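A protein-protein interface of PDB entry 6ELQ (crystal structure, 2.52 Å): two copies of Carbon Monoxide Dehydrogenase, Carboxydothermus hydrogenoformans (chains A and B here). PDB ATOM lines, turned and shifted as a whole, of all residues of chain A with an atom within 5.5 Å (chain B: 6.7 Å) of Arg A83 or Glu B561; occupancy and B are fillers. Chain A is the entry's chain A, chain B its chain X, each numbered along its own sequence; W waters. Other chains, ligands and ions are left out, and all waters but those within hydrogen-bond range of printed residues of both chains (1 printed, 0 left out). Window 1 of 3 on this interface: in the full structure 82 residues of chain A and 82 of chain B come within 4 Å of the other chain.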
ATOM      1  N   ARG A  48     -25.075 -13.385  22.211  1.00  0.00           N
ATOM      2  CA  ARG A  48     -25.014 -13.589  23.651  1.00  0.00           C
ATOM      3  C   ARG A  48     -23.907 -14.571  24.018  1.00  0.00           C
ATOM      4  O   ARG A  48     -23.983 -15.213  25.073  1.00  0.00           O
ATOM      5  CB  ARG A  48     -26.361 -14.086  24.186  1.00  0.00           C
ATOM      6  CG  ARG A  48     -27.505 -13.091  24.039  1.00  0.00           C
ATOM      7  CD  ARG A  48     -28.858 -13.741  24.298  1.00  0.00           C
ATOM      8  NE  ARG A  48     -28.894 -14.462  25.567  1.00  0.00           N
ATOM      9  CZ  ARG A  48     -29.867 -15.294  25.927  1.00  0.00           C
ATOM     10  NH1 ARG A  48     -30.890 -15.514  25.110  1.00  0.00           N
ATOM     11  NH2 ARG A  48     -29.819 -15.910  27.100  1.00  0.00           N
ATOM     12  N   HIS A  49     -22.884 -14.705  23.171  1.00  0.00           N
ATOM     13  CA  HIS A  49     -21.796 -15.649  23.404  1.00  0.00           C
ATOM     14  C   HIS A  49     -20.907 -15.268  24.580  1.00  0.00           C
ATOM     15  O   HIS A  49     -19.988 -16.026  24.908  1.00  0.00           O
ATOM     16  CB  HIS A  49     -20.956 -15.796  22.137  1.00  0.00           C
ATOM     17  CG  HIS A  49     -21.613 -16.628  21.081  1.00  0.00           C
ATOM     18  ND1 HIS A  49     -20.914 -17.220  20.050  1.00  0.00           N
ATOM     19  CD2 HIS A  49     -22.910 -16.980  20.907  1.00  0.00           C
ATOM     20  CE1 HIS A  49     -21.754 -17.892  19.283  1.00  0.00           C
ATOM     21  NE2 HIS A  49     -22.970 -17.764  19.781  1.00  0.00           N
ATOM     22  N   CYS A  50     -21.153 -14.122  25.212  1.00  0.00           N
ATOM     23  CA  CYS A  50     -20.511 -13.778  26.470  1.00  0.00           C
ATOM     24  C   CYS A  50     -21.495 -12.958  27.290  1.00  0.00           C
ATOM     25  O   CYS A  50     -22.524 -12.498  26.787  1.00  0.00           O
ATOM     26  CB  CYS A  50     -19.199 -13.018  26.252  1.00  0.00           C
ATOM     27  SG  CYS A  50     -19.416 -11.293  25.802  1.00  0.00           S
ATOM     28  N   ALA A  78     -22.098 -15.502  11.205  1.00  0.00           N
ATOM     29  CA  ALA A  78     -21.343 -16.701  10.854  1.00  0.00           C
ATOM     30  C   ALA A  78     -20.955 -17.496  12.094  1.00  0.00           C
ATOM     31  O   ALA A  78     -20.996 -18.731  12.082  1.00  0.00           O
ATOM     32  CB  ALA A  78     -20.104 -16.325  10.043  1.00  0.00           C
ATOM     33  N   ARG A  79     -20.574 -16.810  13.174  1.00  0.00           N
ATOM     34  CA  ARG A  79     -20.232 -17.510  14.408  1.00  0.00           C
ATOM     35  C   ARG A  79     -21.451 -18.208  14.998  1.00  0.00           C
ATOM     36  O   ARG A  79     -21.347 -19.333  15.502  1.00  0.00           O
ATOM     37  CB  ARG A  79     -19.626 -16.534  15.414  1.00  0.00           C
ATOM     38  CG  ARG A  79     -19.479 -17.072  16.824  1.00  0.00           C
ATOM     39  CD  ARG A  79     -18.879 -16.011  17.727  1.00  0.00           C
ATOM     40  NE  ARG A  79     -19.673 -14.786  17.745  1.00  0.00           N
ATOM     41  CZ  ARG A  79     -19.234 -13.620  18.211  1.00  0.00           C
ATOM     42  NH1 ARG A  79     -18.004 -13.522  18.692  1.00  0.00           N
ATOM     43  NH2 ARG A  79     -20.019 -12.550  18.192  1.00  0.00           N
ATOM     44  N   ASN A  80     -22.617 -17.560  14.933  1.00  0.00           N
ATOM     45  CA  ASN A  80     -23.845 -18.209  15.381  1.00  0.00           C
ATOM     46  C   ASN A  80     -24.202 -19.393  14.492  1.00  0.00           C
ATOM     47  O   ASN A  80     -24.667 -20.428  14.983  1.00  0.00           O
ATOM     48  CB  ASN A  80     -24.995 -17.204  15.410  1.00  0.00           C
ATOM     49  CG  ASN A  80     -26.301 -17.832  15.855  1.00  0.00           C
ATOM     50  OD1 ASN A  80     -26.592 -17.906  17.048  1.00  0.00           O
ATOM     51  ND2 ASN A  80     -27.094 -18.290  14.896  1.00  0.00           N
ATOM     52  N   LEU A  81     -24.008 -19.257  13.177  1.00  0.00           N
ATOM     53  CA  LEU A  81     -24.340 -20.351  12.270  1.00  0.00           C
ATOM     54  C   LEU A  81     -23.461 -21.569  12.532  1.00  0.00           C
ATOM     55  O   LEU A  81     -23.934 -22.710  12.466  1.00  0.00           O
ATOM     56  CB  LEU A  81     -24.209 -19.889  10.819  1.00  0.00           C
ATOM     57  CG  LEU A  81     -24.445 -20.953   9.743  1.00  0.00           C
ATOM     58  CD1 LEU A  81     -25.842 -21.543   9.853  1.00  0.00           C
ATOM     59  CD2 LEU A  81     -24.208 -20.391   8.349  1.00  0.00           C
ATOM     60  N   LEU A  82     -22.182 -21.346  12.840  1.00  0.00           N
ATOM     61  CA  LEU A  82     -21.290 -22.463  13.136  1.00  0.00           C
ATOM     62  C   LEU A  82     -21.692 -23.167  14.425  1.00  0.00           C
ATOM     63  O   LEU A  82     -21.685 -24.401  14.488  1.00  0.00           O
ATOM     64  CB  LEU A  82     -19.842 -21.974  13.214  1.00  0.00           C
ATOM     65  CG  LEU A  82     -18.783 -22.988  13.659  1.00  0.00           C
ATOM     66  CD1 LEU A  82     -18.770 -24.210  12.753  1.00  0.00           C
ATOM     67  CD2 LEU A  82     -17.405 -22.337  13.704  1.00  0.00           C
ATOM     68  N   ARG A  83     -22.053 -22.405  15.461  1.00  0.00           N
ATOM     69  CA  ARG A  83     -22.432 -23.030  16.726  1.00  0.00           C
ATOM     70  C   ARG A  83     -23.718 -23.834  16.586  1.00  0.00           C
ATOM     71  O   ARG A  83     -23.850 -24.914  17.173  1.00  0.00           O
ATOM     72  CB  ARG A  83     -22.583 -21.974  17.823  1.00  0.00           C
ATOM     73  CG  ARG A  83     -23.065 -22.546  19.154  1.00  0.00           C
ATOM     74  CD  ARG A  83     -23.010 -21.530  20.287  1.00  0.00           C
ATOM     75  NE  ARG A  83     -21.642 -21.198  20.667  1.00  0.00           N
ATOM     76  CZ  ARG A  83     -21.305 -20.621  21.814  1.00  0.00           C
ATOM     77  NH1 ARG A  83     -22.239 -20.314  22.704  1.00  0.00           N
ATOM     78  NH2 ARG A  83     -20.033 -20.358  22.079  1.00  0.00           N
ATOM     79  N   GLN A  84     -24.679 -23.330  15.810  1.00  0.00           N
ATOM     80  CA  GLN A  84     -25.940 -24.040  15.655  1.00  0.00           C
ATOM     81  C   GLN A  84     -25.812 -25.241  14.726  1.00  0.00           C
ATOM     82  O   GLN A  84     -26.476 -26.260  14.951  1.00  0.00           O
ATOM     83  CB  GLN A  84     -27.023 -23.081  15.161  1.00  0.00           C
ATOM     84  CG  GLN A  84     -27.428 -22.052  16.207  1.00  0.00           C
ATOM     85  CD  GLN A  84     -28.723 -21.348  15.869  1.00  0.00           C
ATOM     86  OE1 GLN A  84     -28.800 -20.593  14.899  1.00  0.00           O
ATOM     87  NE2 GLN A  84     -29.753 -21.593  16.671  1.00  0.00           N
ATOM     88  N   VAL A  85     -24.978 -25.148  13.689  1.00  0.00           N
ATOM     89  CA  VAL A  85     -24.702 -26.318  12.860  1.00  0.00           C
ATOM     90  C   VAL A  85     -23.924 -27.357  13.658  1.00  0.00           C
ATOM     91  O   VAL A  85     -24.177 -28.564  13.549  1.00  0.00           O
ATOM     92  CB  VAL A  85     -23.959 -25.902  11.577  1.00  0.00           C
ATOM     93  CG1 VAL A  85     -23.312 -27.107  10.913  1.00  0.00           C
ATOM     94  CG2 VAL A  85     -24.919 -25.218  10.617  1.00  0.00           C
ATOM     95  N   THR A  86     -22.977 -26.902  14.483  1.00  0.00           N
ATOM     96  CA  THR A  86     -22.258 -27.806  15.375  1.00  0.00           C
ATOM     97  C   THR A  86     -23.205 -28.461  16.372  1.00  0.00           C
ATOM     98  O   THR A  86     -23.037 -29.634  16.722  1.00  0.00           O
ATOM     99  CB  THR A  86     -21.149 -27.042  16.105  1.00  0.00           C
ATOM    100  OG1 THR A  86     -20.218 -26.528  15.146  1.00  0.00           O
ATOM    101  CG2 THR A  86     -20.410 -27.943  17.082  1.00  0.00           C
ATOM    102  N   ALA A  87     -24.211 -27.717  16.837  1.00  0.00           N
ATOM    103  CA  ALA A  87     -25.203 -28.293  17.739  1.00  0.00           C
ATOM    104  C   ALA A  87     -26.034 -29.359  17.035  1.00  0.00           C
ATOM    105  O   ALA A  87     -26.306 -30.423  17.606  1.00  0.00           O
ATOM    106  CB  ALA A  87     -26.101 -27.195  18.303  1.00  0.00           C
ATOM    107  N   GLY A  88     -26.452 -29.091  15.797  1.00  0.00           N
ATOM    108  CA  GLY A  88     -27.194 -30.089  15.051  1.00  0.00           C
ATOM    109  C   GLY A  88     -26.358 -31.299  14.690  1.00  0.00           C
ATOM    110  O   GLY A  88     -26.883 -32.413  14.595  1.00  0.00           O
ATOM    111  N   LEU A 193     -17.123 -25.658  18.602  1.00  0.00           N
ATOM    112  CA  LEU A 193     -17.771 -24.964  19.708  1.00  0.00           C
ATOM    113  C   LEU A 193     -16.794 -24.025  20.407  1.00  0.00           C
ATOM    114  O   LEU A 193     -17.173 -22.931  20.842  1.00  0.00           O
ATOM    115  CB  LEU A 193     -18.348 -25.975  20.697  1.00  0.00           C
ATOM    116  CG  LEU A 193     -19.256 -25.401  21.783  1.00  0.00           C
ATOM    117  CD1 LEU A 193     -20.487 -24.762  21.157  1.00  0.00           C
ATOM    118  CD2 LEU A 193     -19.649 -26.482  22.776  1.00  0.00           C
ATOM    119  N   THR A 196     -16.431 -20.785  18.453  1.00  0.00           N
ATOM    120  CA  THR A 196     -17.558 -19.862  18.481  1.00  0.00           C
ATOM    121  C   THR A 196     -17.662 -19.095  19.788  1.00  0.00           C
ATOM    122  O   THR A 196     -18.538 -18.232  19.916  1.00  0.00           O
ATOM    123  CB  THR A 196     -18.876 -20.605  18.221  1.00  0.00           C
ATOM    124  OG1 THR A 196     -19.183 -21.455  19.334  1.00  0.00           O
ATOM    125  CG2 THR A 196     -18.776 -21.436  16.958  1.00  0.00           C
ATOM    126  N   THR A 197     -16.811 -19.388  20.765  1.00  0.00           N
ATOM    127  CA  THR A 197     -16.799 -18.593  21.980  1.00  0.00           C
ATOM    128  C   THR A 197     -16.229 -17.206  21.686  1.00  0.00           C
ATOM    129  O   THR A 197     -15.702 -16.934  20.604  1.00  0.00           O
ATOM    130  CB  THR A 197     -16.000 -19.294  23.077  1.00  0.00           C
ATOM    131  OG1 THR A 197     -14.621 -19.371  22.697  1.00  0.00           O
ATOM    132  CG2 THR A 197     -16.538 -20.703  23.301  1.00  0.00           C
ATOM    133  N   MET A 198     -16.356 -16.316  22.666  1.00  0.00           N
ATOM    134  CA  MET A 198     -15.985 -14.923  22.462  1.00  0.00           C
ATOM    135  C   MET A 198     -14.493 -14.792  22.167  1.00  0.00           C
ATOM    136  O   MET A 198     -13.667 -15.570  22.655  1.00  0.00           O
ATOM    137  CB  MET A 198     -16.372 -14.093  23.692  1.00  0.00           C
ATOM    138  CG  MET A 198     -15.969 -12.626  23.623  1.00  0.00           C
ATOM    139  SD  MET A 198     -14.330 -12.330  24.309  1.00  0.00           S
ATOM    140  CE  MET A 198     -13.824 -10.893  23.366  1.00  0.00           C
ATOM    141  N   GLU A 561     -31.999 -27.341  14.589  1.00  0.00           N
ATOM    142  CA  GLU A 561     -30.605 -27.163  14.206  1.00  0.00           C
ATOM    143  C   GLU A 561     -30.075 -28.360  13.426  1.00  0.00           C
ATOM    144  O   GLU A 561     -29.063 -28.233  12.730  1.00  0.00           O
ATOM    145  CB  GLU A 561     -29.753 -26.901  15.450  1.00  0.00           C
ATOM    146  CG  GLU A 561     -30.227 -25.696  16.261  1.00  0.00           C
ATOM    147  CD  GLU A 561     -29.463 -25.504  17.562  1.00  0.00           C
ATOM    148  OE1 GLU A 561     -28.413 -24.829  17.549  1.00  0.00           O
ATOM    149  OE2 GLU A 561     -29.913 -26.027  18.602  1.00  0.00           O
ATOM    150  N   ASN B  80     -29.963 -22.759  28.300  1.00  0.00           N
ATOM    151  CA  ASN B  80     -28.941 -21.824  27.841  1.00  0.00           C
ATOM    152  C   ASN B  80     -27.686 -21.907  28.701  1.00  0.00           C
ATOM    153  O   ASN B  80     -26.566 -21.835  28.182  1.00  0.00           O
ATOM    154  CB  ASN B  80     -29.490 -20.400  27.841  1.00  0.00           C
ATOM    155  CG  ASN B  80     -28.412 -19.368  27.588  1.00  0.00           C
ATOM    156  OD1 ASN B  80     -27.999 -19.150  26.449  1.00  0.00           O
ATOM    157  ND2 ASN B  80     -27.946 -18.729  28.652  1.00  0.00           N
ATOM    158  N   ARG B  83     -25.608 -24.918  27.577  1.00  0.00           N
ATOM    159  CA  ARG B  83     -24.921 -24.743  26.300  1.00  0.00           C
ATOM    160  C   ARG B  83     -23.706 -23.834  26.445  1.00  0.00           C
ATOM    161  O   ARG B  83     -22.657 -24.089  25.839  1.00  0.00           O
ATOM    162  CB  ARG B  83     -25.885 -24.189  25.249  1.00  0.00           C
ATOM    163  CG  ARG B  83     -25.207 -23.787  23.945  1.00  0.00           C
ATOM    164  CD  ARG B  83     -26.204 -23.544  22.822  1.00  0.00           C
ATOM    165  NE  ARG B  83     -26.912 -24.764  22.450  1.00  0.00           N
ATOM    166  CZ  ARG B  83     -27.502 -24.962  21.275  1.00  0.00           C
ATOM    167  NH1 ARG B  83     -27.464 -24.021  20.342  1.00  0.00           N
ATOM    168  NH2 ARG B  83     -28.119 -26.107  21.029  1.00  0.00           N
ATOM    169  N   GLN B  84     -23.822 -22.774  27.247  1.00  0.00           N
ATOM    170  CA  GLN B  84     -22.703 -21.858  27.422  1.00  0.00           C
ATOM    171  C   GLN B  84     -21.630 -22.436  28.334  1.00  0.00           C
ATOM    172  O   GLN B  84     -20.441 -22.164  28.132  1.00  0.00           O
ATOM    173  CB  GLN B  84     -23.200 -20.518  27.964  1.00  0.00           C
ATOM    174  CG  GLN B  84     -24.234 -19.853  27.071  1.00  0.00           C
ATOM    175  CD  GLN B  84     -24.293 -18.352  27.265  1.00  0.00           C
ATOM    176  OE1 GLN B  84     -25.032 -17.853  28.114  1.00  0.00           O
ATOM    177  NE2 GLN B  84     -23.512 -17.624  26.476  1.00  0.00           N
ATOM    178  N   VAL B  85     -22.018 -23.224  29.339  1.00  0.00           N
ATOM    179  CA  VAL B  85     -21.019 -23.908  30.152  1.00  0.00           C
ATOM    180  C   VAL B  85     -20.303 -24.967  29.322  1.00  0.00           C
ATOM    181  O   VAL B  85     -19.086 -25.153  29.440  1.00  0.00           O
ATOM    182  CB  VAL B  85     -21.671 -24.501  31.415  1.00  0.00           C
ATOM    183  CG1 VAL B  85     -20.790 -25.579  32.027  1.00  0.00           C
ATOM    184  CG2 VAL B  85     -21.932 -23.397  32.429  1.00  0.00           C
ATOM    185  N   THR B  86     -21.044 -25.658  28.452  1.00  0.00           N
ATOM    186  CA  THR B  86     -20.424 -26.607  27.533  1.00  0.00           C
ATOM    187  C   THR B  86     -19.416 -25.914  26.625  1.00  0.00           C
ATOM    188  O   THR B  86     -18.350 -26.468  26.331  1.00  0.00           O
ATOM    189  CB  THR B  86     -21.505 -27.314  26.707  1.00  0.00           C
ATOM    190  OG1 THR B  86     -22.414 -27.992  27.584  1.00  0.00           O
ATOM    191  CG2 THR B  86     -20.893 -28.330  25.755  1.00  0.00           C
ATOM    192  N   ALA B  87     -19.726 -24.691  26.183  1.00  0.00           N
ATOM    193  CA  ALA B  87     -18.824 -23.976  25.286  1.00  0.00           C
ATOM    194  C   ALA B  87     -17.567 -23.509  26.011  1.00  0.00           C
ATOM    195  O   ALA B  87     -16.463 -23.569  25.455  1.00  0.00           O
ATOM    196  CB  ALA B  87     -19.550 -22.791  24.647  1.00  0.00           C
ATOM    197  N   GLY B  88     -17.713 -23.031  27.248  1.00  0.00           N
ATOM    198  CA  GLY B  88     -16.540 -22.675  28.028  1.00  0.00           C
ATOM    199  C   GLY B  88     -15.661 -23.874  28.320  1.00  0.00           C
ATOM    200  O   GLY B  88     -14.431 -23.765  28.343  1.00  0.00           O
ATOM    201  N   ALA B  89     -16.278 -25.038  28.541  1.00  0.00           N
ATOM    202  CA  ALA B  89     -15.500 -26.253  28.756  1.00  0.00           C
ATOM    203  C   ALA B  89     -14.769 -26.667  27.487  1.00  0.00           C
ATOM    204  O   ALA B  89     -13.606 -27.084  27.542  1.00  0.00           O
ATOM    205  CB  ALA B  89     -16.406 -27.383  29.247  1.00  0.00           C
ATOM    206  N   HIS B  92     -11.423 -24.681  27.195  1.00  0.00           N
ATOM    207  CA  HIS B  92     -10.322 -25.177  28.015  1.00  0.00           C
ATOM    208  C   HIS B  92      -9.848 -26.549  27.548  1.00  0.00           C
ATOM    209  O   HIS B  92      -8.639 -26.794  27.463  1.00  0.00           O
ATOM    210  CB  HIS B  92     -10.743 -25.223  29.483  1.00  0.00           C
ATOM    211  CG  HIS B  92     -10.856 -23.874  30.121  1.00  0.00           C
ATOM    212  ND1 HIS B  92     -11.920 -23.515  30.919  1.00  0.00           N
ATOM    213  CD2 HIS B  92     -10.036 -22.798  30.082  1.00  0.00           C
ATOM    214  CE1 HIS B  92     -11.754 -22.275  31.342  1.00  0.00           C
ATOM    215  NE2 HIS B  92     -10.616 -21.817  30.849  1.00  0.00           N
ATOM    216  N   LEU B 193     -24.230 -30.740  24.279  1.00  0.00           N
ATOM    217  CA  LEU B 193     -24.651 -29.864  23.191  1.00  0.00           C
ATOM    218  C   LEU B 193     -25.870 -30.436  22.485  1.00  0.00           C
ATOM    219  O   LEU B 193     -26.778 -29.693  22.094  1.00  0.00           O
ATOM    220  CB  LEU B 193     -23.503 -29.651  22.206  1.00  0.00           C
ATOM    221  CG  LEU B 193     -23.688 -28.532  21.183  1.00  0.00           C
ATOM    222  CD1 LEU B 193     -23.821 -27.183  21.881  1.00  0.00           C
ATOM    223  CD2 LEU B 193     -22.532 -28.522  20.195  1.00  0.00           C
ATOM    224  N   ASP B 218     -14.562 -29.220  32.495  1.00  0.00           N
ATOM    225  CA  ASP B 218     -13.744 -28.022  32.364  1.00  0.00           C
ATOM    226  C   ASP B 218     -12.613 -28.010  33.384  1.00  0.00           C
ATOM    227  O   ASP B 218     -11.492 -27.591  33.072  1.00  0.00           O
ATOM    228  CB  ASP B 218     -14.627 -26.782  32.517  1.00  0.00           C
ATOM    229  CG  ASP B 218     -13.872 -25.493  32.281  1.00  0.00           C
ATOM    230  OD1 ASP B 218     -13.610 -25.166  31.106  1.00  0.00           O
ATOM    231  OD2 ASP B 218     -13.543 -24.806  33.272  1.00  0.00           O
ATOM    232  N   CYS B 446     -12.617 -12.363  34.430  1.00  0.00           N
ATOM    233  CA  CYS B 446     -12.210 -11.419  33.412  1.00  0.00           C
ATOM    234  C   CYS B 446     -12.609  -9.995  33.805  1.00  0.00           C
ATOM    235  O   CYS B 446     -12.835  -9.702  34.990  1.00  0.00           O
ATOM    236  CB  CYS B 446     -12.830 -11.851  32.082  1.00  0.00           C
ATOM    237  SG  CYS B 446     -13.719 -13.437  32.138  1.00  0.00           S
ATOM    238  N   GLN B 559     -16.895 -12.385  32.143  1.00  0.00           N
ATOM    239  CA  GLN B 559     -17.585 -12.135  30.883  1.00  0.00           C
ATOM    240  C   GLN B 559     -17.626 -13.374  29.993  1.00  0.00           C
ATOM    241  O   GLN B 559     -18.650 -13.649  29.360  1.00  0.00           O
ATOM    242  CB  GLN B 559     -16.934 -10.967  30.132  1.00  0.00           C
ATOM    243  CG  GLN B 559     -15.467 -11.166  29.757  1.00  0.00           C
ATOM    244  CD  GLN B 559     -15.276 -11.736  28.362  1.00  0.00           C
ATOM    245  OE1 GLN B 559     -16.234 -11.890  27.604  1.00  0.00           O
ATOM    246  NE2 GLN B 559     -14.030 -12.049  28.017  1.00  0.00           N
ATOM    247  N   HIS B 560     -16.535 -14.131  29.944  1.00  0.00           N
ATOM    248  CA  HIS B 560     -16.410 -15.220  28.984  1.00  0.00           C
ATOM    249  C   HIS B 560     -17.137 -16.468  29.471  1.00  0.00           C
ATOM    250  O   HIS B 560     -17.285 -16.702  30.674  1.00  0.00           O
ATOM    251  CB  HIS B 560     -14.936 -15.541  28.737  1.00  0.00           C
ATOM    252  CG  HIS B 560     -14.676 -16.248  27.443  1.00  0.00           C
ATOM    253  ND1 HIS B 560     -14.760 -17.618  27.309  1.00  0.00           N
ATOM    254  CD2 HIS B 560     -14.317 -15.773  26.225  1.00  0.00           C
ATOM    255  CE1 HIS B 560     -14.472 -17.955  26.064  1.00  0.00           C
ATOM    256  NE2 HIS B 560     -14.198 -16.854  25.387  1.00  0.00           N
ATOM    257  N   GLU B 561     -17.587 -17.282  28.511  1.00  0.00           N
ATOM    258  CA  GLU B 561     -18.201 -18.564  28.844  1.00  0.00           C
ATOM    259  C   GLU B 561     -17.249 -19.474  29.609  1.00  0.00           C
ATOM    260  O   GLU B 561     -17.707 -20.376  30.319  1.00  0.00           O
ATOM    261  CB  GLU B 561     -18.690 -19.260  27.572  1.00  0.00           C
ATOM    262  CG  GLU B 561     -19.902 -18.594  26.938  1.00  0.00           C
ATOM    263  CD  GLU B 561     -20.116 -19.006  25.493  1.00  0.00           C
ATOM    264  OE1 GLU B 561     -21.262 -19.351  25.133  1.00  0.00           O
ATOM    265  OE2 GLU B 561     -19.138 -18.981  24.716  1.00  0.00           O
ATOM    266  N   LYS B 562     -15.938 -19.258  29.480  1.00  0.00           N
ATOM    267  CA  LYS B 562     -14.985 -20.012  30.284  1.00  0.00           C
ATOM    268  C   LYS B 562     -15.158 -19.721  31.767  1.00  0.00           C
ATOM    269  O   LYS B 562     -14.906 -20.596  32.602  1.00  0.00           O
ATOM    270  CB  LYS B 562     -13.555 -19.702  29.842  1.00  0.00           C
ATOM    271  CG  LYS B 562     -13.154 -20.351  28.528  1.00  0.00           C
ATOM    272  CD  LYS B 562     -11.728 -19.986  28.141  1.00  0.00           C
ATOM    273  CE  LYS B 562     -11.622 -18.509  27.798  1.00  0.00           C
ATOM    274  NZ  LYS B 562     -10.222 -18.039  27.597  1.00  0.00           N
ATOM    275  N   ALA B 563     -15.597 -18.509  32.115  1.00  0.00           N
ATOM    276  CA  ALA B 563     -15.808 -18.182  33.521  1.00  0.00           C
ATOM    277  C   ALA B 563     -17.033 -18.891  34.084  1.00  0.00           C
ATOM    278  O   ALA B 563     -17.032 -19.295  35.253  1.00  0.00           O
ATOM    279  CB  ALA B 563     -15.934 -16.670  33.697  1.00  0.00           C
ATOM    280  N   LEU B 564     -18.082 -19.053  33.272  1.00  0.00           N
ATOM    281  CA  LEU B 564     -19.245 -19.815  33.712  1.00  0.00           C
ATOM    282  C   LEU B 564     -18.871 -21.261  34.012  1.00  0.00           C
ATOM    283  O   LEU B 564     -19.307 -21.827  35.023  1.00  0.00           O
ATOM    284  CB  LEU B 564     -20.343 -19.750  32.650  1.00  0.00           C
ATOM    285  CG  LEU B 564     -20.939 -18.372  32.353  1.00  0.00           C
ATOM    286  CD1 LEU B 564     -21.962 -18.444  31.229  1.00  0.00           C
ATOM    287  CD2 LEU B 564     -21.564 -17.780  33.606  1.00  0.00           C
ATOM    288  N   SER B 565     -18.060 -21.874  33.145  1.00  0.00           N
ATOM    289  CA  SER B 565     -17.591 -23.235  33.390  1.00  0.00           C
ATOM    290  C   SER B 565     -16.770 -23.307  34.670  1.00  0.00           C
ATOM    291  O   SER B 565     -16.984 -24.189  35.511  1.00  0.00           O
ATOM    292  CB  SER B 565     -16.762 -23.720  32.202  1.00  0.00           C
ATOM    293  OG  SER B 565     -17.368 -23.364  30.975  1.00  0.00           O
ATOM    294  N   ILE B 566     -15.815 -22.386  34.826  1.00  0.00           N
ATOM    295  CA  ILE B 566     -14.960 -22.381  36.011  1.00  0.00           C
ATOM    296  C   ILE B 566     -15.798 -22.179  37.264  1.00  0.00           C
ATOM    297  O   ILE B 566     -15.628 -22.886  38.266  1.00  0.00           O
ATOM    298  CB  ILE B 566     -13.870 -21.303  35.878  1.00  0.00           C
ATOM    299  CG1 ILE B 566     -12.893 -21.672  34.760  1.00  0.00           C
ATOM    300  CG2 ILE B 566     -13.139 -21.112  37.198  1.00  0.00           C
ATOM    301  CD1 ILE B 566     -11.943 -20.570  34.397  1.00  0.00           C
HETATM  302  O   HOH W   1     -17.681 -16.963  25.427  1.00  0.00           O
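NH2 of Arg B83 lies within salt-bridge range of OE2 of Glu A561, at 3.0 Å.
The side-chain amide nitrogen (NE2) of Gln B84 lies within hydrogen-bond range of the backbone carbonyl oxygen (O) of Arg A48 (2.8 Å).
The side-chain sulfur of Cys A50 lies close to the side-chain amide oxygen of Gln B559 (3.7 Å).
The side-chain amide nitrogen (NE2) of Gln B559 sits at hydrogen-bond distance from the side-chain sulfur (SD) of Met A198, 3.7 Å away.
A ring nitrogen (NE2) of His B560 is in hydrogen-bond range of the backbone carbonyl oxygen (O) of Met A198, at 3.1 Å.
The guanidinium group (NH1) of Arg A83 is in salt-bridge range of the side-chain carboxylate (OE1) of Glu B561 (2.8 Å).
The backbone carbonyl oxygen of His A49 lies close to the side-chain carboxylate of Glu B561, at 3.1 Å.
The side-chain amide nitrogen (ND2) of Asn B80 lies within hydrogen-bond range of the side-chain amide oxygen (OE1) of Gln B84 (3.1 Å).
SG of Cys B446 lies close to N of Gln B559 (3.3 Å).
The side-chain sulfur (SG) of Cys B446 sits close to the backbone NH (N) of His B560 (3.6 Å).
The backbone carbonyl oxygen (O) of Glu B561 is in hydrogen-bond range of the side-chain hydroxyl (OG) of Ser B565, at 3.1 Å.
The backbone carbonyl oxygen (O) of Leu A82 sits at hydrogen-bond distance from the side-chain hydroxyl (OG1) of Thr A86 (2.7 Å).
The guanidinium group of Arg A83 lies within hydrogen-bond range of the side-chain hydroxyl of Thr A196 (2.8 Å).
Asn B80 touches Arg A48 (ND2 to NH2, 3.7 Å).
C of His A49 touches NE2 of Gln B84, at 3.99 Å.
Arg A83 touches Ala B87 (NH2 to CB, 3.6 Å).
O of Thr A86 touches CD2 of Leu B193 (3.7 Å).
Ala A87 touches Leu B193 (CA to CD2, 3.6 Å).
CD2 of Leu A193 touches CG2 of Thr B86 (3.7 Å).
CA of Ala B87 touches CD2 of Leu A193 (3.6 Å).
Thr A197 touches Ala B87 (CG2 to O, 3.6 Å).
CB of Thr A197 touches CE1 of His B560, at 3.6 Å.
Thr A197 touches Glu B561 (CG2 to OE2, 3.4 Å).
Of the printed residues of chain B, Arg A83 touches Ala B87 (3.6 Å) and Glu B561 (2.8 Å).
Val A85 touches none of the printed residues of chain B.
Thr A196 touches none of the printed residues of chain B.
Of the printed residues of chain B, Glu A561 touches Arg B83 (3.0 Å).
Of the printed residues of chain A, Asn B80 touches Arg A48.
Of the printed residues of chain A, Arg B83 touches Ala A87 and Glu A561.
Of the printed residues of chain A, His B560 touches Thr A197 and Met A198.
Of chain A, only His A49, Arg A83 and Thr A197 come within 4 Å of Glu B561.
The nearest residue of chain A that does not touch Glu B561 is Met A198 (4.4 Å).
Of the 20 printed residues of chain B, 9 touch a printed residue of chain A.
Of the 19 printed residues of chain A, 10 touch a printed residue of chain B.
Hydrophobic or aromatic side chains of chain A within 4 Å of the printed part of chain B: Ala A87, Leu A193 and Met A198.
Among the printed residues, 18 pairs touch across the chains.
Among the printed residues, Asp or Glu carboxylates within 4 Å of a Lys or Arg side-chain nitrogen of the other chain: Arg A83 with Glu B561 (2.8 Å) and Glu A561 with Arg B83 (3.0 Å).
Arg A83 touches Ala B87, and with the chains exchanged Ala A87 touches Arg B83.
Arg A83 touches Glu B561, and with the chains exchanged Glu A561 touches Arg B83.
Thr A86 touches Leu B193, and with the chains exchanged Leu A193 touches Thr B86.
Ala A87 touches Leu B193, and with the chains exchanged Leu A193 touches Ala B87.
Water W1 lies within hydrogen-bond range of O of His A49 (2.5 Å), OE2 of Glu B561 (2.6 Å), N of Met A198 (3.1 Å) and NE2 of His B560 (3.5 Å).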
